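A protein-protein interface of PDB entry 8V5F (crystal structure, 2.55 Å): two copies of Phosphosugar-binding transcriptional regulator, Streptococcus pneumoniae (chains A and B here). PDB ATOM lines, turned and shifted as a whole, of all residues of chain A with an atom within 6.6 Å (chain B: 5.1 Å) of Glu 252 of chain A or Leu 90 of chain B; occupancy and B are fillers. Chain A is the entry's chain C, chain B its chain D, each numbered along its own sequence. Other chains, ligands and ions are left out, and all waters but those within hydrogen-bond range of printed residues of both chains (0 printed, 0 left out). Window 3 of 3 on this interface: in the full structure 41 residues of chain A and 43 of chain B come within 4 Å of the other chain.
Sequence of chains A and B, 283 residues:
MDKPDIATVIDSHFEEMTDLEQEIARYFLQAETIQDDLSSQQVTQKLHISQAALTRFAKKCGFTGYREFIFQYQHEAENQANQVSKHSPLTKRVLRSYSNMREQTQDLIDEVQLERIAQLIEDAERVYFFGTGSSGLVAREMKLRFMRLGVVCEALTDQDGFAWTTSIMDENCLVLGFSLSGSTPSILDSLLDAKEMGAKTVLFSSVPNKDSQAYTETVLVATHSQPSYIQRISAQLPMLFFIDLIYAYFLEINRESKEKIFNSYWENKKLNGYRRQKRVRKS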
ATOM      1  N   GLU A 111       9.562  -3.939 -25.298  1.00  0.00           N
ATOM      2  CA  GLU A 111       8.748  -3.936 -24.081  1.00  0.00           C
ATOM      3  C   GLU A 111       7.849  -2.705 -24.008  1.00  0.00           C
ATOM      4  O   GLU A 111       6.655  -2.816 -23.703  1.00  0.00           O
ATOM      5  CB  GLU A 111       9.647  -4.010 -22.847  1.00  0.00           C
ATOM      6  CG  GLU A 111      10.265  -5.373 -22.601  1.00  0.00           C
ATOM      7  CD  GLU A 111      10.280  -5.766 -21.128  1.00  0.00           C
ATOM      8  OE1 GLU A 111      10.166  -4.870 -20.268  1.00  0.00           O
ATOM      9  OE2 GLU A 111      10.388  -6.974 -20.824  1.00  0.00           O
ATOM     10  N   LEU A 245       1.966 -11.700 -24.380  1.00  0.00           N
ATOM     11  CA  LEU A 245       2.741 -10.612 -23.800  1.00  0.00           C
ATOM     12  C   LEU A 245       1.858  -9.395 -23.563  1.00  0.00           C
ATOM     13  O   LEU A 245       1.815  -8.848 -22.453  1.00  0.00           O
ATOM     14  CB  LEU A 245       3.916 -10.268 -24.717  1.00  0.00           C
ATOM     15  CG  LEU A 245       4.996 -11.346 -24.825  1.00  0.00           C
ATOM     16  CD1 LEU A 245       5.950 -11.026 -25.971  1.00  0.00           C
ATOM     17  CD2 LEU A 245       5.772 -11.515 -23.522  1.00  0.00           C
ATOM     18  N   TYR A 247      -1.325  -9.446 -23.383  1.00  0.00           N
ATOM     19  CA  TYR A 247      -2.324  -9.838 -22.398  1.00  0.00           C
ATOM     20  C   TYR A 247      -1.767  -9.722 -20.986  1.00  0.00           C
ATOM     21  O   TYR A 247      -2.472  -9.294 -20.066  1.00  0.00           O
ATOM     22  CB  TYR A 247      -2.815 -11.267 -22.673  1.00  0.00           C
ATOM     23  CG  TYR A 247      -3.791 -11.778 -21.627  1.00  0.00           C
ATOM     24  CD1 TYR A 247      -3.336 -12.332 -20.439  1.00  0.00           C
ATOM     25  CD2 TYR A 247      -5.160 -11.693 -21.818  1.00  0.00           C
ATOM     26  CE1 TYR A 247      -4.210 -12.788 -19.484  1.00  0.00           C
ATOM     27  CE2 TYR A 247      -6.038 -12.152 -20.863  1.00  0.00           C
ATOM     28  CZ  TYR A 247      -5.555 -12.691 -19.698  1.00  0.00           C
ATOM     29  OH  TYR A 247      -6.402 -13.159 -18.729  1.00  0.00           O
ATOM     30  N   ALA A 248      -0.511 -10.129 -20.792  1.00  0.00           N
ATOM     31  CA  ALA A 248       0.095 -10.083 -19.465  1.00  0.00           C
ATOM     32  C   ALA A 248       0.304  -8.645 -19.000  1.00  0.00           C
ATOM     33  O   ALA A 248       0.146  -8.343 -17.811  1.00  0.00           O
ATOM     34  CB  ALA A 248       1.418 -10.850 -19.475  1.00  0.00           C
ATOM     35  N   TYR A 249       0.685  -7.754 -19.915  1.00  0.00           N
ATOM     36  CA  TYR A 249       0.806  -6.342 -19.572  1.00  0.00           C
ATOM     37  C   TYR A 249      -0.567  -5.718 -19.347  1.00  0.00           C
ATOM     38  O   TYR A 249      -0.814  -5.089 -18.311  1.00  0.00           O
ATOM     39  CB  TYR A 249       1.547  -5.615 -20.689  1.00  0.00           C
ATOM     40  CG  TYR A 249       3.048  -5.627 -20.547  1.00  0.00           C
ATOM     41  CD1 TYR A 249       3.870  -5.650 -21.667  1.00  0.00           C
ATOM     42  CD2 TYR A 249       3.650  -5.594 -19.295  1.00  0.00           C
ATOM     43  CE1 TYR A 249       5.253  -5.640 -21.537  1.00  0.00           C
ATOM     44  CE2 TYR A 249       5.021  -5.591 -19.153  1.00  0.00           C
ATOM     45  CZ  TYR A 249       5.822  -5.612 -20.275  1.00  0.00           C
ATOM     46  OH  TYR A 249       7.194  -5.596 -20.127  1.00  0.00           O
ATOM     47  N   PHE A 250      -1.487  -5.918 -20.296  1.00  0.00           N
ATOM     48  CA  PHE A 250      -2.800  -5.288 -20.214  1.00  0.00           C
ATOM     49  C   PHE A 250      -3.590  -5.794 -19.016  1.00  0.00           C
ATOM     50  O   PHE A 250      -4.449  -5.079 -18.491  1.00  0.00           O
ATOM     51  CB  PHE A 250      -3.565  -5.535 -21.520  1.00  0.00           C
ATOM     52  CG  PHE A 250      -5.042  -5.266 -21.430  1.00  0.00           C
ATOM     53  CD1 PHE A 250      -5.540  -3.988 -21.609  1.00  0.00           C
ATOM     54  CD2 PHE A 250      -5.930  -6.290 -21.166  1.00  0.00           C
ATOM     55  CE1 PHE A 250      -6.899  -3.736 -21.519  1.00  0.00           C
ATOM     56  CE2 PHE A 250      -7.293  -6.044 -21.091  1.00  0.00           C
ATOM     57  CZ  PHE A 250      -7.772  -4.757 -21.263  1.00  0.00           C
ATOM     58  N   LEU A 251      -3.320  -7.015 -18.566  1.00  0.00           N
ATOM     59  CA  LEU A 251      -4.021  -7.518 -17.392  1.00  0.00           C
ATOM     60  C   LEU A 251      -3.676  -6.705 -16.150  1.00  0.00           C
ATOM     61  O   LEU A 251      -4.537  -6.506 -15.283  1.00  0.00           O
ATOM     62  CB  LEU A 251      -3.686  -8.995 -17.181  1.00  0.00           C
ATOM     63  CG  LEU A 251      -4.244  -9.626 -15.903  1.00  0.00           C
ATOM     64  CD1 LEU A 251      -5.776  -9.683 -15.939  1.00  0.00           C
ATOM     65  CD2 LEU A 251      -3.649 -11.005 -15.693  1.00  0.00           C
ATOM     66  N   GLU A 252      -2.430  -6.224 -16.048  1.00  0.00           N
ATOM     67  CA  GLU A 252      -1.993  -5.510 -14.849  1.00  0.00           C
ATOM     68  C   GLU A 252      -2.584  -4.105 -14.751  1.00  0.00           C
ATOM     69  O   GLU A 252      -2.646  -3.549 -13.648  1.00  0.00           O
ATOM     70  CB  GLU A 252      -0.460  -5.435 -14.811  1.00  0.00           C
ATOM     71  CG  GLU A 252       0.252  -6.800 -14.758  1.00  0.00           C
ATOM     72  CD  GLU A 252      -0.511  -7.838 -13.954  1.00  0.00           C
ATOM     73  OE1 GLU A 252      -0.674  -7.647 -12.726  1.00  0.00           O
ATOM     74  OE2 GLU A 252      -0.973  -8.833 -14.557  1.00  0.00           O
ATOM     75  N   ILE A 253      -3.021  -3.524 -15.866  1.00  0.00           N
ATOM     76  CA  ILE A 253      -3.693  -2.226 -15.845  1.00  0.00           C
ATOM     77  C   ILE A 253      -5.081  -2.430 -15.251  1.00  0.00           C
ATOM     78  O   ILE A 253      -5.933  -3.082 -15.856  1.00  0.00           O
ATOM     79  CB  ILE A 253      -3.772  -1.606 -17.244  1.00  0.00           C
ATOM     80  CG1 ILE A 253      -2.415  -1.731 -17.945  1.00  0.00           C
ATOM     81  CG2 ILE A 253      -4.184  -0.146 -17.142  1.00  0.00           C
ATOM     82  CD1 ILE A 253      -2.393  -1.180 -19.347  1.00  0.00           C
ATOM     83  N   ASN A 254      -5.306  -1.885 -14.057  1.00  0.00           N
ATOM     84  CA  ASN A 254      -6.579  -2.038 -13.354  1.00  0.00           C
ATOM     85  C   ASN A 254      -6.906  -3.511 -13.128  1.00  0.00           C
ATOM     86  O   ASN A 254      -8.001  -3.981 -13.434  1.00  0.00           O
ATOM     87  CB  ASN A 254      -7.705  -1.343 -14.120  1.00  0.00           C
ATOM     88  CG  ASN A 254      -7.492   0.151 -14.239  1.00  0.00           C
ATOM     89  OD1 ASN A 254      -7.054   0.645 -15.279  1.00  0.00           O
ATOM     90  ND2 ASN A 254      -7.788   0.878 -13.166  1.00  0.00           N
ATOM     91  N   ARG A 255      -5.948  -4.240 -12.556  1.00  0.00           N
ATOM     92  CA  ARG A 255      -6.085  -5.689 -12.455  1.00  0.00           C
ATOM     93  C   ARG A 255      -7.324  -6.085 -11.661  1.00  0.00           C
ATOM     94  O   ARG A 255      -8.053  -7.000 -12.057  1.00  0.00           O
ATOM     95  CB  ARG A 255      -4.829  -6.285 -11.814  1.00  0.00           C
ATOM     96  CG  ARG A 255      -4.966  -7.719 -11.307  1.00  0.00           C
ATOM     97  CD  ARG A 255      -4.296  -8.707 -12.243  1.00  0.00           C
ATOM     98  NE  ARG A 255      -4.416 -10.076 -11.756  1.00  0.00           N
ATOM     99  CZ  ARG A 255      -3.510 -11.021 -11.955  1.00  0.00           C
ATOM    100  NH1 ARG A 255      -2.411 -10.787 -12.656  1.00  0.00           N
ATOM    101  NH2 ARG A 255      -3.710 -12.232 -11.442  1.00  0.00           N
ATOM    102  N   GLU A 256      -7.572  -5.426 -10.530  1.00  0.00           N
ATOM    103  CA  GLU A 256      -8.585  -5.933  -9.611  1.00  0.00           C
ATOM    104  C   GLU A 256      -9.960  -5.974 -10.263  1.00  0.00           C
ATOM    105  O   GLU A 256     -10.694  -6.959 -10.110  1.00  0.00           O
ATOM    106  CB  GLU A 256      -8.617  -5.082  -8.342  1.00  0.00           C
ATOM    107  CG  GLU A 256      -7.723  -5.624  -7.235  1.00  0.00           C
ATOM    108  CD  GLU A 256      -6.249  -5.265  -7.429  1.00  0.00           C
ATOM    109  OE1 GLU A 256      -5.957  -4.272  -8.134  1.00  0.00           O
ATOM    110  OE2 GLU A 256      -5.382  -5.980  -6.874  1.00  0.00           O
ATOM    111  N   LYS A 258     -10.735  -6.128 -13.514  1.00  0.00           N
ATOM    112  CA  LYS A 258     -10.771  -7.158 -14.547  1.00  0.00           C
ATOM    113  C   LYS A 258     -10.870  -8.549 -13.933  1.00  0.00           C
ATOM    114  O   LYS A 258     -11.544  -9.430 -14.477  1.00  0.00           O
ATOM    115  CB  LYS A 258      -9.536  -7.035 -15.441  1.00  0.00           C
ATOM    116  CG  LYS A 258      -9.405  -5.654 -16.096  1.00  0.00           C
ATOM    117  CD  LYS A 258      -8.017  -5.425 -16.650  1.00  0.00           C
ATOM    118  CE  LYS A 258      -8.087  -4.877 -18.067  1.00  0.00           C
ATOM    119  NZ  LYS A 258      -7.546  -3.506 -18.177  1.00  0.00           N
ATOM    120  N   SER B  88      11.276  -7.346 -18.315  1.00  0.00           N
ATOM    121  CA  SER B  88      10.526  -7.150 -17.085  1.00  0.00           C
ATOM    122  C   SER B  88      10.112  -8.510 -16.541  1.00  0.00           C
ATOM    123  O   SER B  88      10.095  -9.495 -17.283  1.00  0.00           O
ATOM    124  CB  SER B  88       9.292  -6.294 -17.346  1.00  0.00           C
ATOM    125  OG  SER B  88       8.361  -7.041 -18.098  1.00  0.00           O
ATOM    126  N   PRO B  89       9.778  -8.596 -15.252  1.00  0.00           N
ATOM    127  CA  PRO B  89       9.263  -9.872 -14.713  1.00  0.00           C
ATOM    128  C   PRO B  89       8.095 -10.445 -15.507  1.00  0.00           C
ATOM    129  O   PRO B  89       8.028 -11.664 -15.718  1.00  0.00           O
ATOM    130  CB  PRO B  89       8.840  -9.508 -13.282  1.00  0.00           C
ATOM    131  CG  PRO B  89       9.554  -8.223 -12.950  1.00  0.00           C
ATOM    132  CD  PRO B  89      10.070  -7.598 -14.208  1.00  0.00           C
ATOM    133  N   LEU B  90       7.176  -9.594 -15.969  1.00  0.00           N
ATOM    134  CA  LEU B  90       6.035 -10.083 -16.740  1.00  0.00           C
ATOM    135  C   LEU B  90       6.475 -10.766 -18.034  1.00  0.00           C
ATOM    136  O   LEU B  90       5.950 -11.827 -18.388  1.00  0.00           O
ATOM    137  CB  LEU B  90       5.080  -8.928 -17.054  1.00  0.00           C
ATOM    138  CG  LEU B  90       4.244  -8.372 -15.903  1.00  0.00           C
ATOM    139  CD1 LEU B  90       3.310  -7.286 -16.421  1.00  0.00           C
ATOM    140  CD2 LEU B  90       3.448  -9.454 -15.194  1.00  0.00           C
ATOM    141  N   THR B  91       7.416 -10.157 -18.768  1.00  0.00           N
ATOM    142  CA  THR B  91       7.925 -10.766 -19.996  1.00  0.00           C
ATOM    143  C   THR B  91       8.617 -12.095 -19.704  1.00  0.00           C
ATOM    144  O   THR B  91       8.394 -13.096 -20.395  1.00  0.00           O
ATOM    145  CB  THR B  91       8.888  -9.802 -20.694  1.00  0.00           C
ATOM    146  OG1 THR B  91       8.224  -8.561 -20.952  1.00  0.00           O
ATOM    147  CG2 THR B  91       9.388 -10.375 -22.002  1.00  0.00           C
ATOM    148  N   LYS B  92       9.455 -12.129 -18.669  1.00  0.00           N
ATOM    149  CA  LYS B  92      10.126 -13.376 -18.325  1.00  0.00           C
ATOM    150  C   LYS B  92       9.112 -14.450 -17.945  1.00  0.00           C
ATOM    151  O   LYS B  92       9.298 -15.630 -18.261  1.00  0.00           O
ATOM    152  CB  LYS B  92      11.137 -13.134 -17.198  1.00  0.00           C
ATOM    153  CG  LYS B  92      12.348 -12.273 -17.616  1.00  0.00           C
ATOM    154  CD  LYS B  92      12.864 -11.349 -16.502  1.00  0.00           C
ATOM    155  CE  LYS B  92      13.097 -12.088 -15.200  1.00  0.00           C
ATOM    156  NZ  LYS B  92      13.646 -11.189 -14.142  1.00  0.00           N
ATOM    157  N   ARG B  93       8.022 -14.064 -17.281  1.00  0.00           N
ATOM    158  CA  ARG B  93       7.029 -15.054 -16.880  1.00  0.00           C
ATOM    159  C   ARG B  93       6.335 -15.671 -18.091  1.00  0.00           C
ATOM    160  O   ARG B  93       6.096 -16.884 -18.136  1.00  0.00           O
ATOM    161  CB  ARG B  93       6.003 -14.413 -15.948  1.00  0.00           C
ATOM    162  CG  ARG B  93       5.055 -15.406 -15.313  1.00  0.00           C
ATOM    163  CD  ARG B  93       3.708 -14.780 -14.990  1.00  0.00           C
ATOM    164  NE  ARG B  93       3.069 -14.236 -16.185  1.00  0.00           N
ATOM    165  CZ  ARG B  93       1.972 -13.487 -16.186  1.00  0.00           C
ATOM    166  NH1 ARG B  93       1.366 -13.145 -15.059  1.00  0.00           N
ATOM    167  NH2 ARG B  93       1.469 -13.072 -17.348  1.00  0.00           N
ATOM    168  N   VAL B  94       5.992 -14.854 -19.079  1.00  0.00           N
ATOM    169  CA  VAL B  94       5.322 -15.374 -20.264  1.00  0.00           C
ATOM    170  C   VAL B  94       6.267 -16.266 -21.056  1.00  0.00           C
ATOM    171  O   VAL B  94       5.900 -17.368 -21.481  1.00  0.00           O
ATOM    172  CB  VAL B  94       4.794 -14.215 -21.124  1.00  0.00           C
ATOM    173  CG1 VAL B  94       4.380 -14.718 -22.486  1.00  0.00           C
ATOM    174  CG2 VAL B  94       3.652 -13.520 -20.411  1.00  0.00           C
ATOM    175  N   GLN B 231      -3.971 -15.987 -15.463  1.00  0.00           N
ATOM    176  CA  GLN B 231      -2.586 -15.671 -15.800  1.00  0.00           C
ATOM    177  C   GLN B 231      -1.968 -16.641 -16.804  1.00  0.00           C
ATOM    178  O   GLN B 231      -0.934 -16.310 -17.399  1.00  0.00           O
ATOM    179  CB  GLN B 231      -1.710 -15.623 -14.534  1.00  0.00           C
ATOM    180  CG  GLN B 231      -1.945 -14.389 -13.656  1.00  0.00           C
ATOM    181  CD  GLN B 231      -0.889 -14.233 -12.581  1.00  0.00           C
ATOM    182  OE1 GLN B 231      -0.197 -13.222 -12.524  1.00  0.00           O
ATOM    183  NE2 GLN B 231      -0.750 -15.247 -11.734  1.00  0.00           N
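OE1 of Gln 231 of chain B is in hydrogen-bond range of NH1 of Arg 255 of chain A, 3.3 Å away. The side-chain carboxylate (OE2) of Glu 111 of chain A is in hydrogen-bond range of the side-chain hydroxyl (OG1) of Thr 91 of chain B (2.7 Å). OG1 of Thr 91 of chain B lies within hydrogen-bond range of OH of Tyr 249 of chain A (3.2 Å). The side-chain hydroxyl of Tyr 249 of chain A sits at hydrogen-bond distance from the side-chain hydroxyl of Ser 88 of chain B, at 2.8 Å. The backbone NH of Ser 88 of chain B sits at hydrogen-bond distance from the side-chain carboxylate of Glu 111 of chain A (2.7 Å).
OG of Ser 88 of chain B sits at hydrogen-bond distance from OG1 of Thr 91 of chain B (3.2 Å). The side-chain carboxylate (OE1) of Glu 111 of chain A is in hydrogen-bond range of the side-chain hydroxyl (OH) of Tyr 249 of chain A. The side-chain carboxylate (OE2) of Glu 252 of chain A is in salt-bridge range of the guanidinium group (NH1) of Arg 255 of chain A (3.1 Å). The side-chain amide oxygen (OE1) of Gln 231 of chain B lies within hydrogen-bond range of the guanidinium group (NH1) of Arg 93 of chain B (3.0 Å).
CG1 of Val 94 of chain B touches CD2 of Leu 245 of chain A, at 3.6 Å. Ala 248 of chain A touches Leu 90 of chain B. CB of Ala 248 of chain A touches NH2 of Arg 93 of chain B (3.1 Å). Ala 248 of chain A touches Val 94 of chain B. Tyr 249 of chain A touches Leu 90 of chain B. CG of Glu 252 of chain A touches CD1 of Leu 90 of chain B, at 3.5 Å.
Of the printed residues of chain B, Glu 111 of chain A touches Ser 88 (2.7 Å) and Thr 91 (2.7 Å). Printed residues of chain B within 4 Å of Leu 245 of chain A: Val 94. Of chain B, only Leu 90 (3.5 Å) comes within 4 Å of Glu 252 of chain A. Leu 90 of chain B touches three residues of chain A. Printed residues of chain A within 4 Å of Arg 93 of chain B: Ala 248. Of the printed residues of chain A, Gln 231 of chain B touches Arg 255. The nearest residue of chain A that does not touch Leu 90 of chain B is Leu 245 of chain A (5.1 Å). The nearest printed residue of chain B that does not touch Arg 255 of chain A is Arg 93 of chain B (5.1 Å).
Of the 13 printed residues of chain A, 6 touch a printed residue of chain B. Hydrophobic or aromatic side chains of chain A that line the printed part of chain B: Leu 245, Ala 248 and Tyr 249. Along chain A the printed residues that touch a printed residue of chain B span positions 111 to 255. Hydrophobic or aromatic side chains of chain B that line the printed part of chain A: Leu 90 and Val 94. Along chain B the printed residues that touch a printed residue of chain A span positions 88 to 231. Among the printed residues, no Asp or Glu carboxylate lies within 4 Å of a Lys or Arg side-chain nitrogen of the other chain.
No position is printed for both chains. Of the 11 pairs that touch across the chains among the printed residues, none has its exchanged pair printed and touching as well.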
